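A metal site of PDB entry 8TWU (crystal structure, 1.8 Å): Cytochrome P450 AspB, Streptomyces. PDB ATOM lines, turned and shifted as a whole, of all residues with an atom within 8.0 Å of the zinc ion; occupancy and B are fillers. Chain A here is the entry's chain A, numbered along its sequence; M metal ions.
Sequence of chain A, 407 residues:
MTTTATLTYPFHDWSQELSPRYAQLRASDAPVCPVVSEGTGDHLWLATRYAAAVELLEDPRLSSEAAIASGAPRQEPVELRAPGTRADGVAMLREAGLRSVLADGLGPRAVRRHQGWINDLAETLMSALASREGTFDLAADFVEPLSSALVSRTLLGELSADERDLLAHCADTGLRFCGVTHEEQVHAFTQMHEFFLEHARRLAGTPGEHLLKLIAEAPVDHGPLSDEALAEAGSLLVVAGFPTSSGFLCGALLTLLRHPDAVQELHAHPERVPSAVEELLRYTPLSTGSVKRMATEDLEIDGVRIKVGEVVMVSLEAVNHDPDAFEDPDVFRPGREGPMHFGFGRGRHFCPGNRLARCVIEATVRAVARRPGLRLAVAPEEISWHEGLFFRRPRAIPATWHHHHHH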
ATOM      1  N   GLN A 264     -10.592  19.365 -17.625  1.00  0.00           N
ATOM      2  CA  GLN A 264     -12.028  19.569 -17.492  1.00  0.00           C
ATOM      3  C   GLN A 264     -12.759  19.262 -18.801  1.00  0.00           C
ATOM      4  O   GLN A 264     -13.876  18.729 -18.786  1.00  0.00           O
ATOM      5  CB  GLN A 264     -12.286  21.011 -17.038  1.00  0.00           C
ATOM      6  CG  GLN A 264     -13.666  21.251 -16.485  1.00  0.00           C
ATOM      7  CD  GLN A 264     -13.761  20.823 -15.049  1.00  0.00           C
ATOM      8  OE1 GLN A 264     -12.833  21.038 -14.264  1.00  0.00           O
ATOM      9  NE2 GLN A 264     -14.878  20.222 -14.690  1.00  0.00           N
ATOM     10  N   HIS A 267     -13.017  15.595 -18.995  1.00  0.00           N
ATOM     11  CA  HIS A 267     -14.004  15.139 -18.029  1.00  0.00           C
ATOM     12  C   HIS A 267     -15.401  15.146 -18.636  1.00  0.00           C
ATOM     13  O   HIS A 267     -16.187  14.209 -18.437  1.00  0.00           O
ATOM     14  CB  HIS A 267     -13.949  16.028 -16.792  1.00  0.00           C
ATOM     15  CG  HIS A 267     -14.993  15.700 -15.785  1.00  0.00           C
ATOM     16  ND1 HIS A 267     -14.922  14.594 -14.968  1.00  0.00           N
ATOM     17  CD2 HIS A 267     -16.148  16.329 -15.470  1.00  0.00           C
ATOM     18  CE1 HIS A 267     -15.979  14.560 -14.181  1.00  0.00           C
ATOM     19  NE2 HIS A 267     -16.737  15.604 -14.460  1.00  0.00           N
ATOM     20  N   ALA A 268     -15.726  16.202 -19.378  1.00  0.00           N
ATOM     21  CA  ALA A 268     -17.026  16.336 -20.014  1.00  0.00           C
ATOM     22  C   ALA A 268     -17.119  15.557 -21.324  1.00  0.00           C
ATOM     23  O   ALA A 268     -18.236  15.215 -21.746  1.00  0.00           O
ATOM     24  CB  ALA A 268     -17.345  17.828 -20.267  1.00  0.00           C
ATOM     25  N   ALA A 369      -9.076  12.455 -15.882  1.00  0.00           N
ATOM     26  CA  ALA A 369     -10.224  13.176 -16.432  1.00  0.00           C
ATOM     27  C   ALA A 369     -11.475  12.922 -15.596  1.00  0.00           C
ATOM     28  O   ALA A 369     -12.336  13.801 -15.460  1.00  0.00           O
ATOM     29  CB  ALA A 369     -10.435  12.783 -17.894  1.00  0.00           C
ATOM     30  N   ARG A 370     -11.571  11.740 -14.982  1.00  0.00           N
ATOM     31  CA  ARG A 370     -12.698  11.475 -14.099  1.00  0.00           C
ATOM     32  C   ARG A 370     -12.689  12.337 -12.828  1.00  0.00           C
ATOM     33  O   ARG A 370     -13.740  12.452 -12.191  1.00  0.00           O
ATOM     34  CB  ARG A 370     -12.722   9.992 -13.739  1.00  0.00           C
ATOM     35  CG  ARG A 370     -12.918   9.143 -14.967  1.00  0.00           C
ATOM     36  CD  ARG A 370     -13.411   7.762 -14.686  1.00  0.00           C
ATOM     37  NE  ARG A 370     -12.244   6.903 -14.642  1.00  0.00           N
ATOM     38  CZ  ARG A 370     -11.911   5.993 -15.556  1.00  0.00           C
ATOM     39  NH1 ARG A 370     -12.680   5.740 -16.608  1.00  0.00           N
ATOM     40  NH2 ARG A 370     -10.777   5.337 -15.406  1.00  0.00           N
ATOM     41  N   PRO A 372     -11.533  15.977 -11.999  1.00  0.00           N
ATOM     42  CA  PRO A 372     -10.943  17.279 -12.333  1.00  0.00           C
ATOM     43  C   PRO A 372     -10.547  18.101 -11.122  1.00  0.00           C
ATOM     44  O   PRO A 372      -9.940  19.171 -11.290  1.00  0.00           O
ATOM     45  CB  PRO A 372     -12.053  17.988 -13.142  1.00  0.00           C
ATOM     46  CG  PRO A 372     -13.306  17.197 -12.875  1.00  0.00           C
ATOM     47  CD  PRO A 372     -12.908  15.812 -12.492  1.00  0.00           C
ATOM     48  N   HIS A 403     -11.364  19.262  -4.893  1.00  0.00           N
ATOM     49  CA  HIS A 403     -12.693  18.723  -4.648  1.00  0.00           C
ATOM     50  C   HIS A 403     -12.676  17.278  -5.110  1.00  0.00           C
ATOM     51  O   HIS A 403     -11.712  16.837  -5.738  1.00  0.00           O
ATOM     52  CB  HIS A 403     -13.796  19.514  -5.368  1.00  0.00           C
ATOM     53  CG  HIS A 403     -13.622  19.565  -6.856  1.00  0.00           C
ATOM     54  ND1 HIS A 403     -13.982  18.522  -7.676  1.00  0.00           N
ATOM     55  CD2 HIS A 403     -13.160  20.545  -7.676  1.00  0.00           C
ATOM     56  CE1 HIS A 403     -13.731  18.833  -8.935  1.00  0.00           C
ATOM     57  NE2 HIS A 403     -13.234  20.064  -8.960  1.00  0.00           N
ATOM     58  N   HIS A 405     -15.152  15.654  -7.044  1.00  0.00           N
ATOM     59  CA  HIS A 405     -16.112  15.334  -8.098  1.00  0.00           C
ATOM     60  C   HIS A 405     -15.517  14.278  -9.019  1.00  0.00           C
ATOM     61  O   HIS A 405     -14.370  14.395  -9.442  1.00  0.00           O
ATOM     62  CB  HIS A 405     -16.473  16.579  -8.882  1.00  0.00           C
ATOM     63  CG  HIS A 405     -17.476  16.328  -9.964  1.00  0.00           C
ATOM     64  ND1 HIS A 405     -18.752  15.891  -9.686  1.00  0.00           N
ATOM     65  CD2 HIS A 405     -17.390  16.427 -11.305  1.00  0.00           C
ATOM     66  CE1 HIS A 405     -19.419  15.741 -10.815  1.00  0.00           C
ATOM     67  NE2 HIS A 405     -18.613  16.059 -11.809  1.00  0.00           N
ATOM     68  N   HIS A 406     -16.295  13.247  -9.329  1.00  0.00           N
ATOM     69  CA  HIS A 406     -15.785  12.179 -10.186  1.00  0.00           C
ATOM     70  C   HIS A 406     -16.932  11.476 -10.906  1.00  0.00           C
ATOM     71  O   HIS A 406     -17.996  11.247 -10.336  1.00  0.00           O
ATOM     72  CB  HIS A 406     -14.943  11.161  -9.389  1.00  0.00           C
ATOM     73  CG  HIS A 406     -15.713  10.348  -8.388  1.00  0.00           C
ATOM     74  ND1 HIS A 406     -16.064  10.842  -7.147  1.00  0.00           N
ATOM     75  CD2 HIS A 406     -16.185   9.079  -8.442  1.00  0.00           C
ATOM     76  CE1 HIS A 406     -16.730   9.909  -6.483  1.00  0.00           C
ATOM     77  NE2 HIS A 406     -16.813   8.830  -7.240  1.00  0.00           N
ATOM     78  N   HIS A 407     -16.696  11.156 -12.182  1.00  0.00           N
ATOM     79  CA  HIS A 407     -17.566  10.270 -12.960  1.00  0.00           C
ATOM     80  C   HIS A 407     -16.961  10.090 -14.359  1.00  0.00           C
ATOM     81  O   HIS A 407     -16.068  10.842 -14.749  1.00  0.00           O
ATOM     82  CB  HIS A 407     -19.005  10.803 -13.056  1.00  0.00           C
ATOM     83  CG  HIS A 407     -19.126  12.143 -13.724  1.00  0.00           C
ATOM     84  ND1 HIS A 407     -19.215  12.294 -15.095  1.00  0.00           N
ATOM     85  CD2 HIS A 407     -19.186  13.398 -13.213  1.00  0.00           C
ATOM     86  CE1 HIS A 407     -19.324  13.574 -15.398  1.00  0.00           C
ATOM     87  NE2 HIS A 407     -19.306  14.266 -14.269  1.00  0.00           N
HETATM   88 ZN    ZN M   1     -18.756  16.502 -14.021  1.00  0.00          ZN
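The backbone carbonyl oxygen of Ala 369 lies within hydrogen-bond range of a ring nitrogen (ND1) of His 267 (2.7 Å). The backbone NH (N) of His 405 is in hydrogen-bond range of a ring nitrogen (ND1) of His 403, at 3.2 Å. The backbone NH (N) of His 407 sits at hydrogen-bond distance from the backbone carbonyl oxygen (O) of Arg 370, at 3.2 Å.
Three residues have an atom within 4 Å of the zinc ion: His 267, His 405 and His 407.
The zinc ion is bound by a ring nitrogen (NE2) of His 267 (2.3 Å), a ring nitrogen (NE2) of His 405 (2.3 Å) and a ring nitrogen (NE2) of His 407 (2.3 Å). The zinc ion has three donor atoms within binding distance.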
